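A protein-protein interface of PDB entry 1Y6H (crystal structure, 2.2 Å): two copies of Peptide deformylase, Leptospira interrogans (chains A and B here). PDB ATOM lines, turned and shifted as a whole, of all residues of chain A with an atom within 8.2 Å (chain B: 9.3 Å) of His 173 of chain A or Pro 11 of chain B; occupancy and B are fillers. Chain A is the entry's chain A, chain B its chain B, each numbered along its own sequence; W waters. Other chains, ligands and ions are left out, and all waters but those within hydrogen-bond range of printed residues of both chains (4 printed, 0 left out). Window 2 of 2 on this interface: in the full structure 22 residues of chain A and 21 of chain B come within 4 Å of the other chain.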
ATOM      1  N   TRP A  98      -2.696  12.295  38.451  1.00  0.00           N
ATOM      2  CA  TRP A  98      -1.505  13.046  38.119  1.00  0.00           C
ATOM      3  C   TRP A  98      -0.877  13.498  39.415  1.00  0.00           C
ATOM      4  O   TRP A  98      -1.183  14.575  39.928  1.00  0.00           O
ATOM      5  CB  TRP A  98      -1.846  14.253  37.248  1.00  0.00           C
ATOM      6  CG  TRP A  98      -2.084  13.875  35.825  1.00  0.00           C
ATOM      7  CD1 TRP A  98      -3.277  13.554  35.246  1.00  0.00           C
ATOM      8  CD2 TRP A  98      -1.090  13.727  34.812  1.00  0.00           C
ATOM      9  NE1 TRP A  98      -3.085  13.215  33.929  1.00  0.00           N
ATOM     10  CE2 TRP A  98      -1.750  13.312  33.638  1.00  0.00           C
ATOM     11  CE3 TRP A  98       0.298  13.906  34.783  1.00  0.00           C
ATOM     12  CZ2 TRP A  98      -1.070  13.071  32.441  1.00  0.00           C
ATOM     13  CZ3 TRP A  98       0.975  13.671  33.594  1.00  0.00           C
ATOM     14  CH2 TRP A  98       0.290  13.257  32.440  1.00  0.00           C
ATOM     15  N   ARG A 108       4.886  16.575  37.553  1.00  0.00           N
ATOM     16  CA  ARG A 108       3.841  15.655  37.923  1.00  0.00           C
ATOM     17  C   ARG A 108       3.783  14.538  36.907  1.00  0.00           C
ATOM     18  O   ARG A 108       4.233  14.679  35.766  1.00  0.00           O
ATOM     19  CB  ARG A 108       2.491  16.357  38.095  1.00  0.00           C
ATOM     20  CG  ARG A 108       1.983  17.172  36.943  1.00  0.00           C
ATOM     21  CD  ARG A 108       0.622  17.742  37.341  1.00  0.00           C
ATOM     22  NE  ARG A 108      -0.046  18.415  36.235  1.00  0.00           N
ATOM     23  CZ  ARG A 108       0.046  19.715  35.983  1.00  0.00           C
ATOM     24  NH1 ARG A 108       0.782  20.494  36.764  1.00  0.00           N
ATOM     25  NH2 ARG A 108      -0.602  20.231  34.948  1.00  0.00           N
ATOM     26  N   LYS A 161       5.876   9.008  29.213  1.00  0.00           N
ATOM     27  CA  LYS A 161       5.308  10.006  28.318  1.00  0.00           C
ATOM     28  C   LYS A 161       4.273  10.838  29.081  1.00  0.00           C
ATOM     29  O   LYS A 161       3.997  11.974  28.713  1.00  0.00           O
ATOM     30  CB  LYS A 161       4.655   9.347  27.097  1.00  0.00           C
ATOM     31  CG  LYS A 161       5.648   8.651  26.169  1.00  0.00           C
ATOM     32  CD  LYS A 161       4.996   8.225  24.856  1.00  0.00           C
ATOM     33  CE  LYS A 161       3.961   7.121  25.050  1.00  0.00           C
ATOM     34  NZ  LYS A 161       4.600   5.809  25.369  1.00  0.00           N
ATOM     35  N   LEU A 162       3.710  10.270  30.146  1.00  0.00           N
ATOM     36  CA  LEU A 162       2.717  10.968  30.968  1.00  0.00           C
ATOM     37  C   LEU A 162       3.460  11.494  32.184  1.00  0.00           C
ATOM     38  O   LEU A 162       3.224  11.065  33.319  1.00  0.00           O
ATOM     39  CB  LEU A 162       1.617  10.004  31.401  1.00  0.00           C
ATOM     40  CG  LEU A 162       0.825   9.398  30.241  1.00  0.00           C
ATOM     41  CD1 LEU A 162      -0.110   8.319  30.760  1.00  0.00           C
ATOM     42  CD2 LEU A 162       0.051  10.496  29.523  1.00  0.00           C
ATOM     43  N   PHE A 165       6.673  18.901  33.188  1.00  0.00           N
ATOM     44  CA  PHE A 165       6.613  20.060  34.057  1.00  0.00           C
ATOM     45  C   PHE A 165       5.220  20.631  34.107  1.00  0.00           C
ATOM     46  O   PHE A 165       4.530  20.717  33.094  1.00  0.00           O
ATOM     47  CB  PHE A 165       7.606  21.114  33.597  1.00  0.00           C
ATOM     48  CG  PHE A 165       9.013  20.626  33.598  1.00  0.00           C
ATOM     49  CD1 PHE A 165       9.494  19.876  32.535  1.00  0.00           C
ATOM     50  CD2 PHE A 165       9.847  20.868  34.687  1.00  0.00           C
ATOM     51  CE1 PHE A 165      10.786  19.367  32.545  1.00  0.00           C
ATOM     52  CE2 PHE A 165      11.151  20.360  34.711  1.00  0.00           C
ATOM     53  CZ  PHE A 165      11.622  19.608  33.638  1.00  0.00           C
ATOM     54  N   ASN A 166       4.822  21.020  35.307  1.00  0.00           N
ATOM     55  CA  ASN A 166       3.500  21.561  35.534  1.00  0.00           C
ATOM     56  C   ASN A 166       3.067  22.610  34.535  1.00  0.00           C
ATOM     57  O   ASN A 166       2.036  22.467  33.888  1.00  0.00           O
ATOM     58  CB  ASN A 166       3.427  22.114  36.948  1.00  0.00           C
ATOM     59  CG  ASN A 166       3.787  21.076  37.971  1.00  0.00           C
ATOM     60  OD1 ASN A 166       3.398  19.915  37.842  1.00  0.00           O
ATOM     61  ND2 ASN A 166       4.526  21.477  38.995  1.00  0.00           N
ATOM     62  N   GLU A 167       3.860  23.662  34.394  1.00  0.00           N
ATOM     63  CA  GLU A 167       3.501  24.728  33.478  1.00  0.00           C
ATOM     64  C   GLU A 167       3.453  24.266  32.030  1.00  0.00           C
ATOM     65  O   GLU A 167       2.634  24.752  31.257  1.00  0.00           O
ATOM     66  CB  GLU A 167       4.449  25.914  33.666  1.00  0.00           C
ATOM     67  CG  GLU A 167       4.232  26.607  35.012  1.00  0.00           C
ATOM     68  CD  GLU A 167       5.254  27.691  35.313  1.00  0.00           C
ATOM     69  OE1 GLU A 167       5.427  28.603  34.477  1.00  0.00           O
ATOM     70  OE2 GLU A 167       5.881  27.635  36.397  1.00  0.00           O
ATOM     71  N   THR A 168       4.308  23.319  31.653  1.00  0.00           N
ATOM     72  CA  THR A 168       4.268  22.830  30.279  1.00  0.00           C
ATOM     73  C   THR A 168       3.031  21.956  30.101  1.00  0.00           C
ATOM     74  O   THR A 168       2.328  22.070  29.102  1.00  0.00           O
ATOM     75  CB  THR A 168       5.521  22.024  29.909  1.00  0.00           C
ATOM     76  OG1 THR A 168       6.659  22.887  29.925  1.00  0.00           O
ATOM     77  CG2 THR A 168       5.383  21.443  28.509  1.00  0.00           C
ATOM     78  N   LEU A 169       2.769  21.088  31.072  1.00  0.00           N
ATOM     79  CA  LEU A 169       1.599  20.219  31.022  1.00  0.00           C
ATOM     80  C   LEU A 169       0.313  21.052  31.045  1.00  0.00           C
ATOM     81  O   LEU A 169      -0.645  20.735  30.343  1.00  0.00           O
ATOM     82  CB  LEU A 169       1.608  19.242  32.206  1.00  0.00           C
ATOM     83  CG  LEU A 169       2.687  18.159  32.177  1.00  0.00           C
ATOM     84  CD1 LEU A 169       2.752  17.439  33.507  1.00  0.00           C
ATOM     85  CD2 LEU A 169       2.388  17.173  31.044  1.00  0.00           C
ATOM     86  N   ASP A 170       0.293  22.113  31.851  1.00  0.00           N
ATOM     87  CA  ASP A 170      -0.883  22.973  31.936  1.00  0.00           C
ATOM     88  C   ASP A 170      -1.177  23.621  30.590  1.00  0.00           C
ATOM     89  O   ASP A 170      -2.284  23.501  30.066  1.00  0.00           O
ATOM     90  CB  ASP A 170      -0.697  24.098  32.970  1.00  0.00           C
ATOM     91  CG  ASP A 170      -0.526  23.583  34.386  1.00  0.00           C
ATOM     92  OD1 ASP A 170      -1.194  22.596  34.750  1.00  0.00           O
ATOM     93  OD2 ASP A 170       0.271  24.181  35.146  1.00  0.00           O
ATOM     94  N   SER A 171      -0.174  24.294  30.029  1.00  0.00           N
ATOM     95  CA  SER A 171      -0.332  25.001  28.765  1.00  0.00           C
ATOM     96  C   SER A 171      -0.464  24.145  27.511  1.00  0.00           C
ATOM     97  O   SER A 171      -0.722  24.673  26.426  1.00  0.00           O
ATOM     98  CB  SER A 171       0.814  25.998  28.574  1.00  0.00           C
ATOM     99  OG  SER A 171       2.051  25.339  28.413  1.00  0.00           O
ATOM    100  N   SER A 172      -0.299  22.836  27.646  1.00  0.00           N
ATOM    101  CA  SER A 172      -0.406  21.949  26.495  1.00  0.00           C
ATOM    102  C   SER A 172      -1.709  21.154  26.535  1.00  0.00           C
ATOM    103  O   SER A 172      -2.141  20.587  25.531  1.00  0.00           O
ATOM    104  CB  SER A 172       0.795  21.002  26.455  1.00  0.00           C
ATOM    105  OG  SER A 172       2.005  21.734  26.304  1.00  0.00           O
ATOM    106  N   HIS A 173      -2.335  21.124  27.704  1.00  0.00           N
ATOM    107  CA  HIS A 173      -3.588  20.412  27.882  1.00  0.00           C
ATOM    108  C   HIS A 173      -4.544  21.316  28.630  1.00  0.00           C
ATOM    109  O   HIS A 173      -4.702  21.207  29.846  1.00  0.00           O
ATOM    110  CB  HIS A 173      -3.351  19.121  28.658  1.00  0.00           C
ATOM    111  CG  HIS A 173      -2.432  18.174  27.954  1.00  0.00           C
ATOM    112  ND1 HIS A 173      -1.076  18.135  28.194  1.00  0.00           N
ATOM    113  CD2 HIS A 173      -2.662  17.297  26.950  1.00  0.00           C
ATOM    114  CE1 HIS A 173      -0.511  17.278  27.364  1.00  0.00           C
ATOM    115  NE2 HIS A 173      -1.451  16.756  26.597  1.00  0.00           N
ATOM    116  N   ASN A 174      -5.185  22.206  27.882  1.00  0.00           N
ATOM    117  CA  ASN A 174      -6.104  23.169  28.458  1.00  0.00           C
ATOM    118  C   ASN A 174      -7.526  22.672  28.639  1.00  0.00           C
ATOM    119  O   ASN A 174      -7.980  21.758  27.948  1.00  0.00           O
ATOM    120  CB  ASN A 174      -6.103  24.435  27.607  1.00  0.00           C
ATOM    121  CG  ASN A 174      -4.715  25.016  27.447  1.00  0.00           C
ATOM    122  OD1 ASN A 174      -4.071  25.396  28.431  1.00  0.00           O
ATOM    123  ND2 ASN A 174      -4.238  25.076  26.206  1.00  0.00           N
ATOM    124  N   VAL A 175      -8.211  23.292  29.595  1.00  0.00           N
ATOM    125  CA  VAL A 175      -9.594  22.978  29.918  1.00  0.00           C
ATOM    126  C   VAL A 175     -10.303  24.304  30.190  1.00  0.00           C
ATOM    127  O   VAL A 175      -9.690  25.369  30.088  1.00  0.00           O
ATOM    128  CB  VAL A 175      -9.697  22.057  31.165  1.00  0.00           C
ATOM    129  CG1 VAL A 175      -9.085  20.695  30.853  1.00  0.00           C
ATOM    130  CG2 VAL A 175      -8.988  22.691  32.354  1.00  0.00           C
ATOM    131  N   LEU A 176     -11.585  24.241  30.538  1.00  0.00           N
ATOM    132  CA  LEU A 176     -12.358  25.447  30.805  1.00  0.00           C
ATOM    133  C   LEU A 176     -11.913  26.172  32.067  1.00  0.00           C
ATOM    134  O   LEU A 176     -12.706  26.876  32.684  1.00  0.00           O
ATOM    135  CB  LEU A 176     -13.843  25.117  30.932  1.00  0.00           C
ATOM    136  CG  LEU A 176     -14.798  25.885  30.023  1.00  0.00           C
ATOM    137  CD1 LEU A 176     -16.201  25.747  30.585  1.00  0.00           C
ATOM    138  CD2 LEU A 176     -14.401  27.347  29.935  1.00  0.00           C
ATOM    139  N   ASP A 177     -10.655  25.996  32.457  1.00  0.00           N
ATOM    140  CA  ASP A 177     -10.136  26.661  33.647  1.00  0.00           C
ATOM    141  C   ASP A 177     -10.160  28.163  33.393  1.00  0.00           C
ATOM    142  O   ASP A 177     -10.596  28.562  32.290  1.00  0.00           O
ATOM    143  CB  ASP A 177      -8.698  26.221  33.929  1.00  0.00           C
ATOM    144  CG  ASP A 177      -7.740  26.616  32.818  1.00  0.00           C
ATOM    145  OD1 ASP A 177      -7.887  26.087  31.696  1.00  0.00           O
ATOM    146  OD2 ASP A 177      -6.848  27.458  33.059  1.00  0.00           O
ATOM    147  OXT ASP A 177      -9.734  28.918  34.291  1.00  0.00           O
ATOM    148  N   LEU B   6      11.222  23.480  23.862  1.00  0.00           N
ATOM    149  CA  LEU B   6      10.057  22.846  24.455  1.00  0.00           C
ATOM    150  C   LEU B   6      10.496  21.942  25.592  1.00  0.00           C
ATOM    151  O   LEU B   6      11.503  21.241  25.486  1.00  0.00           O
ATOM    152  CB  LEU B   6       9.299  22.037  23.400  1.00  0.00           C
ATOM    153  CG  LEU B   6       8.904  22.826  22.145  1.00  0.00           C
ATOM    154  CD1 LEU B   6       8.122  21.936  21.193  1.00  0.00           C
ATOM    155  CD2 LEU B   6       8.081  24.041  22.546  1.00  0.00           C
ATOM    156  N   ARG B   7       9.743  21.962  26.685  1.00  0.00           N
ATOM    157  CA  ARG B   7      10.079  21.135  27.831  1.00  0.00           C
ATOM    158  C   ARG B   7       9.276  19.846  27.865  1.00  0.00           C
ATOM    159  O   ARG B   7       8.229  19.727  27.223  1.00  0.00           O
ATOM    160  CB  ARG B   7       9.861  21.910  29.129  1.00  0.00           C
ATOM    161  CG  ARG B   7      10.738  23.132  29.276  1.00  0.00           C
ATOM    162  CD  ARG B   7      10.643  23.702  30.685  1.00  0.00           C
ATOM    163  NE  ARG B   7       9.266  24.004  31.067  1.00  0.00           N
ATOM    164  CZ  ARG B   7       8.895  24.373  32.289  1.00  0.00           C
ATOM    165  NH1 ARG B   7       9.802  24.488  33.253  1.00  0.00           N
ATOM    166  NH2 ARG B   7       7.617  24.622  32.551  1.00  0.00           N
ATOM    167  N   MET B   8       9.782  18.878  28.618  1.00  0.00           N
ATOM    168  CA  MET B   8       9.114  17.596  28.752  1.00  0.00           C
ATOM    169  C   MET B   8       7.686  17.856  29.195  1.00  0.00           C
ATOM    170  O   MET B   8       7.439  18.659  30.095  1.00  0.00           O
ATOM    171  CB  MET B   8       9.843  16.724  29.771  1.00  0.00           C
ATOM    172  CG  MET B   8       9.212  15.365  29.981  1.00  0.00           C
ATOM    173  SD  MET B   8      10.291  14.286  30.919  1.00  0.00           S
ATOM    174  CE  MET B   8      10.177  14.984  32.508  1.00  0.00           C
ATOM    175  N   GLY B   9       6.754  17.174  28.545  1.00  0.00           N
ATOM    176  CA  GLY B   9       5.349  17.356  28.837  1.00  0.00           C
ATOM    177  C   GLY B   9       4.656  17.869  27.584  1.00  0.00           C
ATOM    178  O   GLY B   9       3.456  17.656  27.397  1.00  0.00           O
ATOM    179  N   ASP B  10       5.416  18.552  26.731  1.00  0.00           N
ATOM    180  CA  ASP B  10       4.893  19.091  25.476  1.00  0.00           C
ATOM    181  C   ASP B  10       4.792  17.921  24.494  1.00  0.00           C
ATOM    182  O   ASP B  10       5.795  17.279  24.166  1.00  0.00           O
ATOM    183  CB  ASP B  10       5.843  20.153  24.925  1.00  0.00           C
ATOM    184  CG  ASP B  10       5.262  20.903  23.743  1.00  0.00           C
ATOM    185  OD1 ASP B  10       4.747  20.253  22.805  1.00  0.00           O
ATOM    186  OD2 ASP B  10       5.329  22.148  23.747  1.00  0.00           O
ATOM    187  N   PRO B  11       3.579  17.630  24.012  1.00  0.00           N
ATOM    188  CA  PRO B  11       3.323  16.535  23.073  1.00  0.00           C
ATOM    189  C   PRO B  11       4.242  16.469  21.860  1.00  0.00           C
ATOM    190  O   PRO B  11       4.528  15.383  21.361  1.00  0.00           O
ATOM    191  CB  PRO B  11       1.861  16.753  22.678  1.00  0.00           C
ATOM    192  CG  PRO B  11       1.267  17.360  23.914  1.00  0.00           C
ATOM    193  CD  PRO B  11       2.334  18.367  24.306  1.00  0.00           C
ATOM    194  N   ILE B  12       4.700  17.622  21.383  1.00  0.00           N
ATOM    195  CA  ILE B  12       5.568  17.658  20.211  1.00  0.00           C
ATOM    196  C   ILE B  12       6.816  16.813  20.410  1.00  0.00           C
ATOM    197  O   ILE B  12       7.247  16.103  19.503  1.00  0.00           O
ATOM    198  CB  ILE B  12       5.996  19.107  19.862  1.00  0.00           C
ATOM    199  CG1 ILE B  12       4.771  19.949  19.489  1.00  0.00           C
ATOM    200  CG2 ILE B  12       6.969  19.097  18.690  1.00  0.00           C
ATOM    201  CD1 ILE B  12       4.039  19.451  18.264  1.00  0.00           C
ATOM    202  N   LEU B  13       7.389  16.894  21.602  1.00  0.00           N
ATOM    203  CA  LEU B  13       8.596  16.151  21.935  1.00  0.00           C
ATOM    204  C   LEU B  13       8.413  14.645  21.814  1.00  0.00           C
ATOM    205  O   LEU B  13       9.391  13.891  21.799  1.00  0.00           O
ATOM    206  CB  LEU B  13       9.038  16.503  23.359  1.00  0.00           C
ATOM    207  CG  LEU B  13      10.056  17.629  23.588  1.00  0.00           C
ATOM    208  CD1 LEU B  13      10.104  18.584  22.416  1.00  0.00           C
ATOM    209  CD2 LEU B  13       9.697  18.348  24.878  1.00  0.00           C
ATOM    210  N   ARG B  14       7.165  14.200  21.733  1.00  0.00           N
ATOM    211  CA  ARG B  14       6.893  12.773  21.614  1.00  0.00           C
ATOM    212  C   ARG B  14       6.392  12.352  20.236  1.00  0.00           C
ATOM    213  O   ARG B  14       5.999  11.203  20.047  1.00  0.00           O
ATOM    214  CB  ARG B  14       5.892  12.331  22.684  1.00  0.00           C
ATOM    215  CG  ARG B  14       6.534  11.809  23.966  1.00  0.00           C
ATOM    216  CD  ARG B  14       7.477  12.818  24.596  1.00  0.00           C
ATOM    217  NE  ARG B  14       7.954  12.371  25.902  1.00  0.00           N
ATOM    218  CZ  ARG B  14       8.758  11.328  26.105  1.00  0.00           C
ATOM    219  NH1 ARG B  14       9.187  10.607  25.085  1.00  0.00           N
ATOM    220  NH2 ARG B  14       9.138  11.010  27.335  1.00  0.00           N
ATOM    221  N   LYS B  15       6.411  13.273  19.275  1.00  0.00           N
ATOM    222  CA  LYS B  15       5.964  12.961  17.916  1.00  0.00           C
ATOM    223  C   LYS B  15       7.149  12.459  17.097  1.00  0.00           C
ATOM    224  O   LYS B  15       8.301  12.550  17.526  1.00  0.00           O
ATOM    225  CB  LYS B  15       5.386  14.201  17.222  1.00  0.00           C
ATOM    226  CG  LYS B  15       4.293  14.936  17.983  1.00  0.00           C
ATOM    227  CD  LYS B  15       3.034  14.107  18.123  1.00  0.00           C
ATOM    228  CE  LYS B  15       1.942  14.894  18.847  1.00  0.00           C
ATOM    229  NZ  LYS B  15       0.702  14.081  19.015  1.00  0.00           N
ATOM    230  N   ILE B  16       6.861  11.932  15.912  1.00  0.00           N
ATOM    231  CA  ILE B  16       7.904  11.431  15.031  1.00  0.00           C
ATOM    232  C   ILE B  16       8.287  12.563  14.092  1.00  0.00           C
ATOM    233  O   ILE B  16       7.424  13.266  13.583  1.00  0.00           O
ATOM    234  CB  ILE B  16       7.411  10.238  14.172  1.00  0.00           C
ATOM    235  CG1 ILE B  16       6.966   9.079  15.067  1.00  0.00           C
ATOM    236  CG2 ILE B  16       8.532   9.770  13.250  1.00  0.00           C
ATOM    237  CD1 ILE B  16       8.093   8.449  15.847  1.00  0.00           C
ATOM    238  N   PRO B  52      12.723  18.931  16.747  1.00  0.00           N
ATOM    239  CA  PRO B  52      11.484  18.871  17.529  1.00  0.00           C
ATOM    240  C   PRO B  52      11.564  19.640  18.849  1.00  0.00           C
ATOM    241  O   PRO B  52      10.555  20.146  19.338  1.00  0.00           O
ATOM    242  CB  PRO B  52      11.249  17.365  17.715  1.00  0.00           C
ATOM    243  CG  PRO B  52      12.600  16.746  17.483  1.00  0.00           C
ATOM    244  CD  PRO B  52      13.181  17.583  16.377  1.00  0.00           C
ATOM    245  N   GLY B  55      10.143  22.717  18.319  1.00  0.00           N
ATOM    246  CA  GLY B  55       8.852  22.614  17.656  1.00  0.00           C
ATOM    247  C   GLY B  55       8.794  22.203  16.197  1.00  0.00           C
ATOM    248  O   GLY B  55       7.714  22.176  15.608  1.00  0.00           O
ATOM    249  N   LEU B  57       9.125  19.296  13.598  1.00  0.00           N
ATOM    250  CA  LEU B  57       9.190  17.849  13.459  1.00  0.00           C
ATOM    251  C   LEU B  57       9.894  17.402  12.183  1.00  0.00           C
ATOM    252  O   LEU B  57       9.287  16.797  11.299  1.00  0.00           O
ATOM    253  CB  LEU B  57       7.781  17.261  13.519  1.00  0.00           C
ATOM    254  CG  LEU B  57       7.123  17.369  14.893  1.00  0.00           C
ATOM    255  CD1 LEU B  57       5.661  16.943  14.807  1.00  0.00           C
ATOM    256  CD2 LEU B  57       7.891  16.501  15.881  1.00  0.00           C
ATOM    257  N   HIS B 147      15.309  11.976  19.966  1.00  0.00           N
ATOM    258  CA  HIS B 147      14.394  13.099  19.854  1.00  0.00           C
ATOM    259  C   HIS B 147      13.587  13.031  18.570  1.00  0.00           C
ATOM    260  O   HIS B 147      12.409  13.400  18.547  1.00  0.00           O
ATOM    261  CB  HIS B 147      15.159  14.419  19.871  1.00  0.00           C
ATOM    262  CG  HIS B 147      15.476  14.919  21.242  1.00  0.00           C
ATOM    263  ND1 HIS B 147      14.522  15.238  22.186  1.00  0.00           N
ATOM    264  CD2 HIS B 147      16.672  15.204  21.814  1.00  0.00           C
ATOM    265  CE1 HIS B 147      15.153  15.695  23.268  1.00  0.00           C
ATOM    266  NE2 HIS B 147      16.458  15.693  23.090  1.00  0.00           N
ATOM    267  N   GLN B 149      12.586  10.478  17.182  1.00  0.00           N
ATOM    268  CA  GLN B 149      11.627   9.382  17.326  1.00  0.00           C
ATOM    269  C   GLN B 149      10.663   9.679  18.464  1.00  0.00           C
ATOM    270  O   GLN B 149       9.895   8.810  18.876  1.00  0.00           O
ATOM    271  CB  GLN B 149      12.354   8.074  17.635  1.00  0.00           C
ATOM    272  CG  GLN B 149      13.340   7.653  16.572  1.00  0.00           C
ATOM    273  CD  GLN B 149      12.679   6.943  15.418  1.00  0.00           C
ATOM    274  OE1 GLN B 149      11.667   7.401  14.876  1.00  0.00           O
ATOM    275  NE2 GLN B 149      13.255   5.813  15.023  1.00  0.00           N
ATOM    276  N   GLY B 150      10.716  10.906  18.976  1.00  0.00           N
ATOM    277  CA  GLY B 150       9.844  11.290  20.069  1.00  0.00           C
ATOM    278  C   GLY B 150      10.247  10.637  21.379  1.00  0.00           C
ATOM    279  O   GLY B 150       9.409  10.381  22.244  1.00  0.00           O
ATOM    280  N   ILE B 151      11.539  10.371  21.532  1.00  0.00           N
ATOM    281  CA  ILE B 151      12.050   9.738  22.738  1.00  0.00           C
ATOM    282  C   ILE B 151      12.986  10.649  23.513  1.00  0.00           C
ATOM    283  O   ILE B 151      13.877  11.275  22.937  1.00  0.00           O
ATOM    284  CB  ILE B 151      12.800   8.446  22.386  1.00  0.00           C
ATOM    285  CG1 ILE B 151      11.823   7.443  21.772  1.00  0.00           C
ATOM    286  CG2 ILE B 151      13.483   7.868  23.626  1.00  0.00           C
ATOM    287  CD1 ILE B 151      12.490   6.177  21.260  1.00  0.00           C
ATOM    288  N   LEU B 152      12.768  10.724  24.824  1.00  0.00           N
ATOM    289  CA  LEU B 152      13.600  11.533  25.713  1.00  0.00           C
ATOM    290  C   LEU B 152      14.407  10.554  26.555  1.00  0.00           C
ATOM    291  O   LEU B 152      14.016   9.397  26.696  1.00  0.00           O
ATOM    292  CB  LEU B 152      12.721  12.406  26.605  1.00  0.00           C
ATOM    293  CG  LEU B 152      11.803  13.405  25.893  1.00  0.00           C
ATOM    294  CD1 LEU B 152      11.034  14.201  26.939  1.00  0.00           C
ATOM    295  CD2 LEU B 152      12.623  14.344  25.012  1.00  0.00           C
HETATM  296  O   HOH W   1       2.098  22.876  24.051  1.00  0.00           O
HETATM  297  O   HOH W   2       7.188  12.948  28.895  1.00  0.00           O
HETATM  298  O   HOH W   3       5.033  13.841  26.867  1.00  0.00           O
HETATM  299  O   HOH W   4       7.577  24.030  27.259  1.00  0.00           O
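The backbone NH (N) of Phe 165 of chain A sits at hydrogen-bond distance from the backbone carbonyl oxygen (O) of Met 8 of chain B, 3.2 Å away. The side-chain hydroxyl (OG1) of Thr 168 of chain A lies within hydrogen-bond range of the guanidinium group (NE) of Arg 7 of chain B, 3.1 Å away.
The backbone carbonyl oxygen (O) of Glu 167 of chain A lies within hydrogen-bond range of the side-chain hydroxyl (OG) of Ser 171 of chain A (3.0 Å). The side-chain hydroxyl of Ser 171 of chain A lies within hydrogen-bond range of the backbone carbonyl oxygen of Thr 168 of chain A. O of Thr 168 of chain A lies within hydrogen-bond range of OG of Ser 172 of chain A (2.8 Å). O of Leu 169 of chain A is in hydrogen-bond range of ND1 of His 173 of chain A (3.4 Å). The side-chain carboxylate (OD1) of Asp 10 of chain B is in hydrogen-bond range of the backbone NH (N) of Ile 12 of chain B (3.0 Å). O of Gly 150 of chain B lies within hydrogen-bond range of NH1 of Arg 14 of chain B, at 2.9 Å.
Among the printed residues, pairs that only touch across the chains: Thr 168 of chain A with Asp 10 of chain B, Glu 167 of chain A with Arg 7 of chain B, Phe 165 of chain A with Arg 7 of chain B, Leu 169 of chain A with Gly 9 of chain B, Ser 172 of chain A with Pro 11 of chain B, Thr 168 of chain A with Gly 9 of chain B, Thr 168 of chain A with Met 8 of chain B, His 173 of chain A with Pro 11 of chain B, Lys 161 of chain A with Arg 14 of chain B and His 173 of chain A with Gly 9 of chain B.
Of the printed residues of chain B, His 173 of chain A touches Gly 9 (3.99 Å) and Pro 11 (3.9 Å). No residue of chain B comes within 4 Å of Asn 174 of chain A. Printed residues of chain B within 4 Å of Ser 172 of chain A: Pro 11 (3.7 Å). Printed residues of chain B within 4 Å of Lys 161 of chain A: Arg 14. Printed residues of chain B within 4 Å of Leu 169 of chain A: Gly 9. Val 175 of chain A touches none of the printed residues of chain B. The nearest residue of chain A that does not touch Pro 11 of chain B is Thr 168 of chain A (6.0 Å).
Printed residues of chain A that touch a printed residue of chain B: Lys 161, Phe 165, Glu 167, Thr 168, Leu 169, Ser 172 and His 173. Hydrophobic or aromatic side chains of chain A that line the printed part of chain B: Phe 165, Leu 169 and His 173. Among the printed residues, 12 pairs touch across the chains.
No position is printed for both chains.
Water W1 bridges the side-chain hydroxyl of Ser 172 of chain A (2.5 Å) and the side-chain carboxylate of Asp 10 of chain B (3.3 Å). Water W3 bridges the backbone carbonyl oxygen (O) of Lys 161 of chain A (2.8 Å) and the guanidinium group (NE) of Arg 14 of chain B (3.4 Å). Water W4 lies within hydrogen-bond range of OG1 of Thr 168 of chain A (3.0 Å) and N of Arg 7 of chain B (3.0 Å). Water W2 lies within hydrogen-bond range of NE of Arg 14 of chain B (3.1 Å) and O of Lys 161 of chain A (3.3 Å).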
